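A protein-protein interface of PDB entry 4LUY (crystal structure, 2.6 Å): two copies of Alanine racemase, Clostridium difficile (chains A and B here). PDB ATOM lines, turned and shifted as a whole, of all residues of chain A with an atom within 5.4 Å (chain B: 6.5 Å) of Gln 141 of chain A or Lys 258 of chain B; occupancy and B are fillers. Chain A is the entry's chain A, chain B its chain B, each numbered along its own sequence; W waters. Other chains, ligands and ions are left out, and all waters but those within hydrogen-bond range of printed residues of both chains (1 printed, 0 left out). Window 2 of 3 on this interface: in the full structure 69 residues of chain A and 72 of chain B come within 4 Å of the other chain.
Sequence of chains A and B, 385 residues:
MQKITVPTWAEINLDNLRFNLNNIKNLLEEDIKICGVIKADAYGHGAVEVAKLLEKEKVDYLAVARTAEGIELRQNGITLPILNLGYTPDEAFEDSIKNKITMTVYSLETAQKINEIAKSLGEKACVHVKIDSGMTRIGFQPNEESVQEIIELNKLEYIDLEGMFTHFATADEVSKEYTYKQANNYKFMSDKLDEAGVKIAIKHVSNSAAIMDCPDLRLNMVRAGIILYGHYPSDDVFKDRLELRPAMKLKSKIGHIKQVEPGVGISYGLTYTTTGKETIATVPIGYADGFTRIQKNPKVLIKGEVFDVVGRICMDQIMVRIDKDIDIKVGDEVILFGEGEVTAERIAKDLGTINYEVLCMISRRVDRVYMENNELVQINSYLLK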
ATOM      1  N   ASP A 132      11.572  13.299   4.528  1.00  0.00           N
ATOM      2  CA  ASP A 132      12.316  12.084   4.349  1.00  0.00           C
ATOM      3  C   ASP A 132      12.460  11.493   5.698  1.00  0.00           C
ATOM      4  O   ASP A 132      13.133  11.999   6.516  1.00  0.00           O
ATOM      5  CB  ASP A 132      13.705  12.380   3.790  1.00  0.00           C
ATOM      6  CG  ASP A 132      14.513  11.144   3.479  1.00  0.00           C
ATOM      7  OD1 ASP A 132      14.222  10.090   3.990  1.00  0.00           O
ATOM      8  OD2 ASP A 132      15.465  11.229   2.729  1.00  0.00           O
ATOM      9  N   THR A 136      14.815   7.537   2.159  1.00  0.00           N
ATOM     10  CA  THR A 136      15.932   8.198   1.568  1.00  0.00           C
ATOM     11  C   THR A 136      15.740   8.539   0.100  1.00  0.00           C
ATOM     12  O   THR A 136      16.660   8.483  -0.666  1.00  0.00           O
ATOM     13  CB  THR A 136      17.161   7.331   1.797  1.00  0.00           C
ATOM     14  OG1 THR A 136      17.046   6.750   3.071  1.00  0.00           O
ATOM     15  CG2 THR A 136      18.358   8.108   1.797  1.00  0.00           C
ATOM     16  N   ARG A 137      14.537   8.899  -0.292  1.00  0.00           N
ATOM     17  CA  ARG A 137      14.259   9.123  -1.698  1.00  0.00           C
ATOM     18  C   ARG A 137      14.160  10.586  -1.993  1.00  0.00           C
ATOM     19  O   ARG A 137      15.080  11.150  -2.534  1.00  0.00           O
ATOM     20  CB  ARG A 137      13.003   8.367  -2.127  1.00  0.00           C
ATOM     21  CG  ARG A 137      12.672   8.440  -3.597  1.00  0.00           C
ATOM     22  CD  ARG A 137      11.571   7.489  -4.010  1.00  0.00           C
ATOM     23  NE  ARG A 137      10.353   7.774  -3.293  1.00  0.00           N
ATOM     24  CZ  ARG A 137       9.250   7.058  -3.321  1.00  0.00           C
ATOM     25  NH1 ARG A 137       9.140   5.990  -4.032  1.00  0.00           N
ATOM     26  NH2 ARG A 137       8.256   7.445  -2.619  1.00  0.00           N
ATOM     27  N   ILE A 138      13.062  11.194  -1.606  1.00  0.00           N
ATOM     28  CA  ILE A 138      12.918  12.615  -1.670  1.00  0.00           C
ATOM     29  C   ILE A 138      12.380  13.078  -0.357  1.00  0.00           C
ATOM     30  O   ILE A 138      11.854  12.302   0.344  1.00  0.00           O
ATOM     31  CB  ILE A 138      12.080  13.088  -2.860  1.00  0.00           C
ATOM     32  CG1 ILE A 138      10.740  12.401  -2.904  1.00  0.00           C
ATOM     33  CG2 ILE A 138      12.834  12.905  -4.143  1.00  0.00           C
ATOM     34  CD1 ILE A 138       9.625  13.266  -3.417  1.00  0.00           C
ATOM     35  N   GLY A 139      12.575  14.331  -0.016  1.00  0.00           N
ATOM     36  CA  GLY A 139      12.113  14.898   1.232  1.00  0.00           C
ATOM     37  C   GLY A 139      13.104  15.678   2.055  1.00  0.00           C
ATOM     38  O   GLY A 139      14.240  15.629   1.832  1.00  0.00           O
ATOM     39  N   PHE A 140      12.628  16.450   2.999  1.00  0.00           N
ATOM     40  CA  PHE A 140      13.490  17.150   3.921  1.00  0.00           C
ATOM     41  C   PHE A 140      14.061  16.145   4.879  1.00  0.00           C
ATOM     42  O   PHE A 140      13.397  15.208   5.208  1.00  0.00           O
ATOM     43  CB  PHE A 140      12.697  18.173   4.739  1.00  0.00           C
ATOM     44  CG  PHE A 140      12.375  19.447   4.021  1.00  0.00           C
ATOM     45  CD1 PHE A 140      13.229  20.498   4.061  1.00  0.00           C
ATOM     46  CD2 PHE A 140      11.204  19.594   3.350  1.00  0.00           C
ATOM     47  CE1 PHE A 140      12.951  21.654   3.413  1.00  0.00           C
ATOM     48  CE2 PHE A 140      10.914  20.754   2.715  1.00  0.00           C
ATOM     49  CZ  PHE A 140      11.789  21.787   2.739  1.00  0.00           C
ATOM     50  N   GLN A 141      15.280  16.327   5.330  1.00  0.00           N
ATOM     51  CA  GLN A 141      15.759  15.558   6.453  1.00  0.00           C
ATOM     52  C   GLN A 141      15.122  16.059   7.709  1.00  0.00           C
ATOM     53  O   GLN A 141      14.994  17.233   7.908  1.00  0.00           O
ATOM     54  CB  GLN A 141      17.240  15.650   6.620  1.00  0.00           C
ATOM     55  CG  GLN A 141      18.093  14.912   5.643  1.00  0.00           C
ATOM     56  CD  GLN A 141      17.562  13.611   5.137  1.00  0.00           C
ATOM     57  OE1 GLN A 141      17.435  12.664   5.858  1.00  0.00           O
ATOM     58  NE2 GLN A 141      17.329  13.551   3.865  1.00  0.00           N
ATOM     59  N   PRO A 142      14.718  15.161   8.570  1.00  0.00           N
ATOM     60  CA  PRO A 142      13.944  15.543   9.722  1.00  0.00           C
ATOM     61  C   PRO A 142      14.827  16.027  10.834  1.00  0.00           C
ATOM     62  O   PRO A 142      15.189  15.329  11.736  1.00  0.00           O
ATOM     63  CB  PRO A 142      13.282  14.252  10.124  1.00  0.00           C
ATOM     64  CG  PRO A 142      14.100  13.185   9.555  1.00  0.00           C
ATOM     65  CD  PRO A 142      15.062  13.748   8.599  1.00  0.00           C
ATOM     66  N   ASN A 143      15.143  17.289  10.735  1.00  0.00           N
ATOM     67  CA  ASN A 143      15.999  17.952  11.641  1.00  0.00           C
ATOM     68  C   ASN A 143      15.511  19.358  11.815  1.00  0.00           C
ATOM     69  O   ASN A 143      14.705  19.814  11.085  1.00  0.00           O
ATOM     70  CB  ASN A 143      17.405  17.890  11.124  1.00  0.00           C
ATOM     71  CG  ASN A 143      17.622  18.725   9.903  1.00  0.00           C
ATOM     72  OD1 ASN A 143      17.334  19.872   9.896  1.00  0.00           O
ATOM     73  ND2 ASN A 143      18.199  18.152   8.899  1.00  0.00           N
ATOM     74  N   SER A 146      15.665  21.875   8.995  1.00  0.00           N
ATOM     75  CA  SER A 146      14.559  21.652   8.116  1.00  0.00           C
ATOM     76  C   SER A 146      13.317  22.347   8.585  1.00  0.00           C
ATOM     77  O   SER A 146      12.607  22.896   7.822  1.00  0.00           O
ATOM     78  CB  SER A 146      14.324  20.178   7.980  1.00  0.00           C
ATOM     79  OG  SER A 146      15.187  19.643   7.043  1.00  0.00           O
ATOM     80  N   MET A 189       8.661  16.269  13.178  1.00  0.00           N
ATOM     81  CA  MET A 189       8.492  17.409  12.335  1.00  0.00           C
ATOM     82  C   MET A 189       7.190  18.099  12.548  1.00  0.00           C
ATOM     83  O   MET A 189       7.104  19.251  12.509  1.00  0.00           O
ATOM     84  CB  MET A 189       8.647  17.006  10.887  1.00  0.00           C
ATOM     85  CG  MET A 189      10.053  16.701  10.454  1.00  0.00           C
ATOM     86  SD  MET A 189      11.210  18.010  10.648  1.00  0.00           S
ATOM     87  CE  MET A 189      10.697  19.241   9.538  1.00  0.00           C
ATOM     88  N   HIS B 256      16.786  15.260  -7.051  1.00  0.00           N
ATOM     89  CA  HIS B 256      17.237  15.519  -5.727  1.00  0.00           C
ATOM     90  C   HIS B 256      18.622  14.990  -5.532  1.00  0.00           C
ATOM     91  O   HIS B 256      18.994  14.030  -6.116  1.00  0.00           O
ATOM     92  CB  HIS B 256      16.273  14.939  -4.714  1.00  0.00           C
ATOM     93  CG  HIS B 256      16.508  15.405  -3.320  1.00  0.00           C
ATOM     94  ND1 HIS B 256      16.800  16.706  -3.021  1.00  0.00           N
ATOM     95  CD2 HIS B 256      16.524  14.745  -2.149  1.00  0.00           C
ATOM     96  CE1 HIS B 256      16.984  16.830  -1.728  1.00  0.00           C
ATOM     97  NE2 HIS B 256      16.819  15.654  -1.176  1.00  0.00           N
ATOM     98  N   ILE B 257      19.402  15.698  -4.749  1.00  0.00           N
ATOM     99  CA  ILE B 257      20.708  15.268  -4.340  1.00  0.00           C
ATOM    100  C   ILE B 257      20.932  15.603  -2.881  1.00  0.00           C
ATOM    101  O   ILE B 257      20.546  16.639  -2.437  1.00  0.00           O
ATOM    102  CB  ILE B 257      21.790  15.837  -5.261  1.00  0.00           C
ATOM    103  CG1 ILE B 257      23.147  15.673  -4.674  1.00  0.00           C
ATOM    104  CG2 ILE B 257      21.556  17.275  -5.539  1.00  0.00           C
ATOM    105  CD1 ILE B 257      23.728  14.357  -5.043  1.00  0.00           C
ATOM    106  N   LYS B 258      21.528  14.689  -2.143  1.00  0.00           N
ATOM    107  CA  LYS B 258      21.746  14.855  -0.719  1.00  0.00           C
ATOM    108  C   LYS B 258      22.803  13.935  -0.151  1.00  0.00           C
ATOM    109  O   LYS B 258      23.154  12.951  -0.724  1.00  0.00           O
ATOM    110  CB  LYS B 258      20.454  14.680   0.047  1.00  0.00           C
ATOM    111  CG  LYS B 258      19.741  13.397  -0.240  1.00  0.00           C
ATOM    112  CD  LYS B 258      19.166  12.831   1.004  1.00  0.00           C
ATOM    113  CE  LYS B 258      18.667  11.438   0.772  1.00  0.00           C
ATOM    114  NZ  LYS B 258      17.794  11.251  -0.379  1.00  0.00           N
ATOM    115  N   GLN B 259      23.251  14.256   1.042  1.00  0.00           N
ATOM    116  CA  GLN B 259      24.199  13.453   1.783  1.00  0.00           C
ATOM    117  C   GLN B 259      23.570  12.620   2.825  1.00  0.00           C
ATOM    118  O   GLN B 259      22.782  13.078   3.588  1.00  0.00           O
ATOM    119  CB  GLN B 259      25.160  14.332   2.486  1.00  0.00           C
ATOM    120  CG  GLN B 259      25.884  15.198   1.525  1.00  0.00           C
ATOM    121  CD  GLN B 259      27.157  14.584   1.113  1.00  0.00           C
ATOM    122  OE1 GLN B 259      27.965  14.217   1.945  1.00  0.00           O
ATOM    123  NE2 GLN B 259      27.359  14.476  -0.166  1.00  0.00           N
ATOM    124  N   VAL B 260      23.955  11.369   2.836  1.00  0.00           N
ATOM    125  CA  VAL B 260      23.325  10.393   3.649  1.00  0.00           C
ATOM    126  C   VAL B 260      24.326   9.784   4.586  1.00  0.00           C
ATOM    127  O   VAL B 260      25.391   9.423   4.195  1.00  0.00           O
ATOM    128  CB  VAL B 260      22.670   9.353   2.766  1.00  0.00           C
ATOM    129  CG1 VAL B 260      21.922   8.334   3.551  1.00  0.00           C
ATOM    130  CG2 VAL B 260      21.750  10.037   1.832  1.00  0.00           C
ATOM    131  N   GLU B 278      27.646   8.866   1.998  1.00  0.00           N
ATOM    132  CA  GLU B 278      27.461   8.698   0.600  1.00  0.00           C
ATOM    133  C   GLU B 278      26.645   9.829   0.025  1.00  0.00           C
ATOM    134  O   GLU B 278      25.754  10.337   0.641  1.00  0.00           O
ATOM    135  CB  GLU B 278      26.774   7.369   0.331  1.00  0.00           C
ATOM    136  CG  GLU B 278      27.730   6.209   0.232  1.00  0.00           C
ATOM    137  CD  GLU B 278      27.100   4.887  -0.071  1.00  0.00           C
ATOM    138  OE1 GLU B 278      26.067   4.830  -0.696  1.00  0.00           O
ATOM    139  OE2 GLU B 278      27.669   3.884   0.294  1.00  0.00           O
ATOM    140  N   THR B 279      26.955  10.204  -1.193  1.00  0.00           N
ATOM    141  CA  THR B 279      26.154  11.139  -1.925  1.00  0.00           C
ATOM    142  C   THR B 279      25.125  10.455  -2.792  1.00  0.00           C
ATOM    143  O   THR B 279      25.444   9.685  -3.636  1.00  0.00           O
ATOM    144  CB  THR B 279      27.017  11.971  -2.812  1.00  0.00           C
ATOM    145  OG1 THR B 279      27.994  12.573  -2.014  1.00  0.00           O
ATOM    146  CG2 THR B 279      26.267  13.009  -3.417  1.00  0.00           C
ATOM    147  N   ILE B 280      23.873  10.772  -2.543  1.00  0.00           N
ATOM    148  CA  ILE B 280      22.775  10.178  -3.215  1.00  0.00           C
ATOM    149  C   ILE B 280      21.904  11.134  -4.005  1.00  0.00           C
ATOM    150  O   ILE B 280      21.316  12.033  -3.496  1.00  0.00           O
ATOM    151  CB  ILE B 280      21.940   9.427  -2.210  1.00  0.00           C
ATOM    152  CG1 ILE B 280      22.774   8.391  -1.516  1.00  0.00           C
ATOM    153  CG2 ILE B 280      20.798   8.754  -2.882  1.00  0.00           C
ATOM    154  CD1 ILE B 280      23.274   7.313  -2.413  1.00  0.00           C
ATOM    155  N   ALA B 281      21.778  10.835  -5.275  1.00  0.00           N
ATOM    156  CA  ALA B 281      20.908  11.511  -6.193  1.00  0.00           C
ATOM    157  C   ALA B 281      19.671  10.711  -6.582  1.00  0.00           C
ATOM    158  O   ALA B 281      19.744   9.599  -6.951  1.00  0.00           O
ATOM    159  CB  ALA B 281      21.695  11.867  -7.413  1.00  0.00           C
ATOM    160  N   THR B 282      18.532  11.341  -6.500  1.00  0.00           N
ATOM    161  CA  THR B 282      17.331  10.740  -6.926  1.00  0.00           C
ATOM    162  C   THR B 282      16.976  11.170  -8.303  1.00  0.00           C
ATOM    163  O   THR B 282      17.025  12.298  -8.617  1.00  0.00           O
ATOM    164  CB  THR B 282      16.189  11.091  -6.015  1.00  0.00           C
ATOM    165  OG1 THR B 282      16.578  10.819  -4.698  1.00  0.00           O
ATOM    166  CG2 THR B 282      15.088  10.259  -6.323  1.00  0.00           C
ATOM    167  N   MET B 319      17.466   5.899  -7.292  1.00  0.00           N
ATOM    168  CA  MET B 319      18.480   6.506  -6.537  1.00  0.00           C
ATOM    169  C   MET B 319      19.816   6.028  -7.015  1.00  0.00           C
ATOM    170  O   MET B 319      19.986   4.918  -7.364  1.00  0.00           O
ATOM    171  CB  MET B 319      18.247   6.308  -5.065  1.00  0.00           C
ATOM    172  CG  MET B 319      17.114   7.156  -4.575  1.00  0.00           C
ATOM    173  SD  MET B 319      15.837   6.179  -3.856  1.00  0.00           S
ATOM    174  CE  MET B 319      14.852   5.668  -5.194  1.00  0.00           C
HETATM  175  O   HOH W   1      15.446  13.043   0.460  1.00  0.00           O
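The side-chain carboxylate (OD2) of Asp 132 of chain A is in salt-bridge range of the side-chain amino group (NZ) of Lys 258 of chain B (3.9 Å). O of Thr 136 of chain A lies within hydrogen-bond range of NZ of Lys 258 of chain B (3.0 Å). O of Arg 137 of chain A lies within hydrogen-bond range of NZ of Lys 258 of chain B, at 3.5 Å. The backbone carbonyl oxygen of Arg 137 of chain A sits at hydrogen-bond distance from the side-chain hydroxyl of Thr 282 of chain B, at 2.7 Å.
OD1 of Asp 132 of chain A lies within hydrogen-bond range of N of Thr 136 of chain A (3.2 Å). NE2 of Gln 141 of chain A lies within hydrogen-bond range of OD2 of Asp 132 of chain A, 3.2 Å away. O of Gln 141 of chain A sits at hydrogen-bond distance from OG of Ser 146 of chain A (2.6 Å). The backbone carbonyl oxygen (O) of His 256 of chain B is in hydrogen-bond range of the backbone NH (N) of Thr 282 of chain B (2.8 Å). O of Lys 258 of chain B lies within hydrogen-bond range of N of Ile 280 of chain B, at 2.9 Å. The backbone NH (N) of Val 260 of chain B is in hydrogen-bond range of the backbone carbonyl oxygen (O) of Glu 278 of chain B, at 3.0 Å.
Among the printed residues, merely in contact across the chains: Gln 141 of chain A with Lys 258 of chain B, Arg 137 of chain A with Met 319 of chain B, Arg 137 of chain A with His 256 of chain B, Thr 136 of chain A with Val 260 of chain B and Gly 139 of chain A with His 256 of chain B.
Gln 141 of chain A touches just one residue of chain B: Lys 258. Of the printed residues of chain A, Val 260 of chain B touches Thr 136. Of the printed residues of chain B, Arg 137 of chain A touches His 256 (3.9 Å), Lys 258 (3.5 Å), Thr 282 (2.7 Å) and Met 319 (3.9 Å). Of the printed residues of chain B, Thr 136 of chain A touches Lys 258 and Val 260. Of the printed residues of chain B, Gly 139 of chain A touches His 256 (3.96 Å). The nearest residue of chain B that does not touch Gln 141 of chain A is Gln 259 of chain B (5.4 Å). The nearest residue of chain A that does not touch Lys 258 of chain B is Ile 138 of chain A (4.9 Å).
Of the 11 printed residues of chain A, 5 touch a printed residue of chain B. Of the 11 printed residues of chain B, 5 touch a printed residue of chain A. Hydrophobic or aromatic side chains of chain B within 4 Å of the printed part of chain A: His 256, Val 260 and Met 319.
No position is printed for both chains.
Water W1 lies within hydrogen-bond range of the side-chain carboxylate (OD2) of Asp 132 of chain A, the side-chain amino group (NZ) of Lys 258 of chain B, the backbone carbonyl oxygen (O) of Gly 139 of chain A and a ring nitrogen (NE2) of His 256 of chain B.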
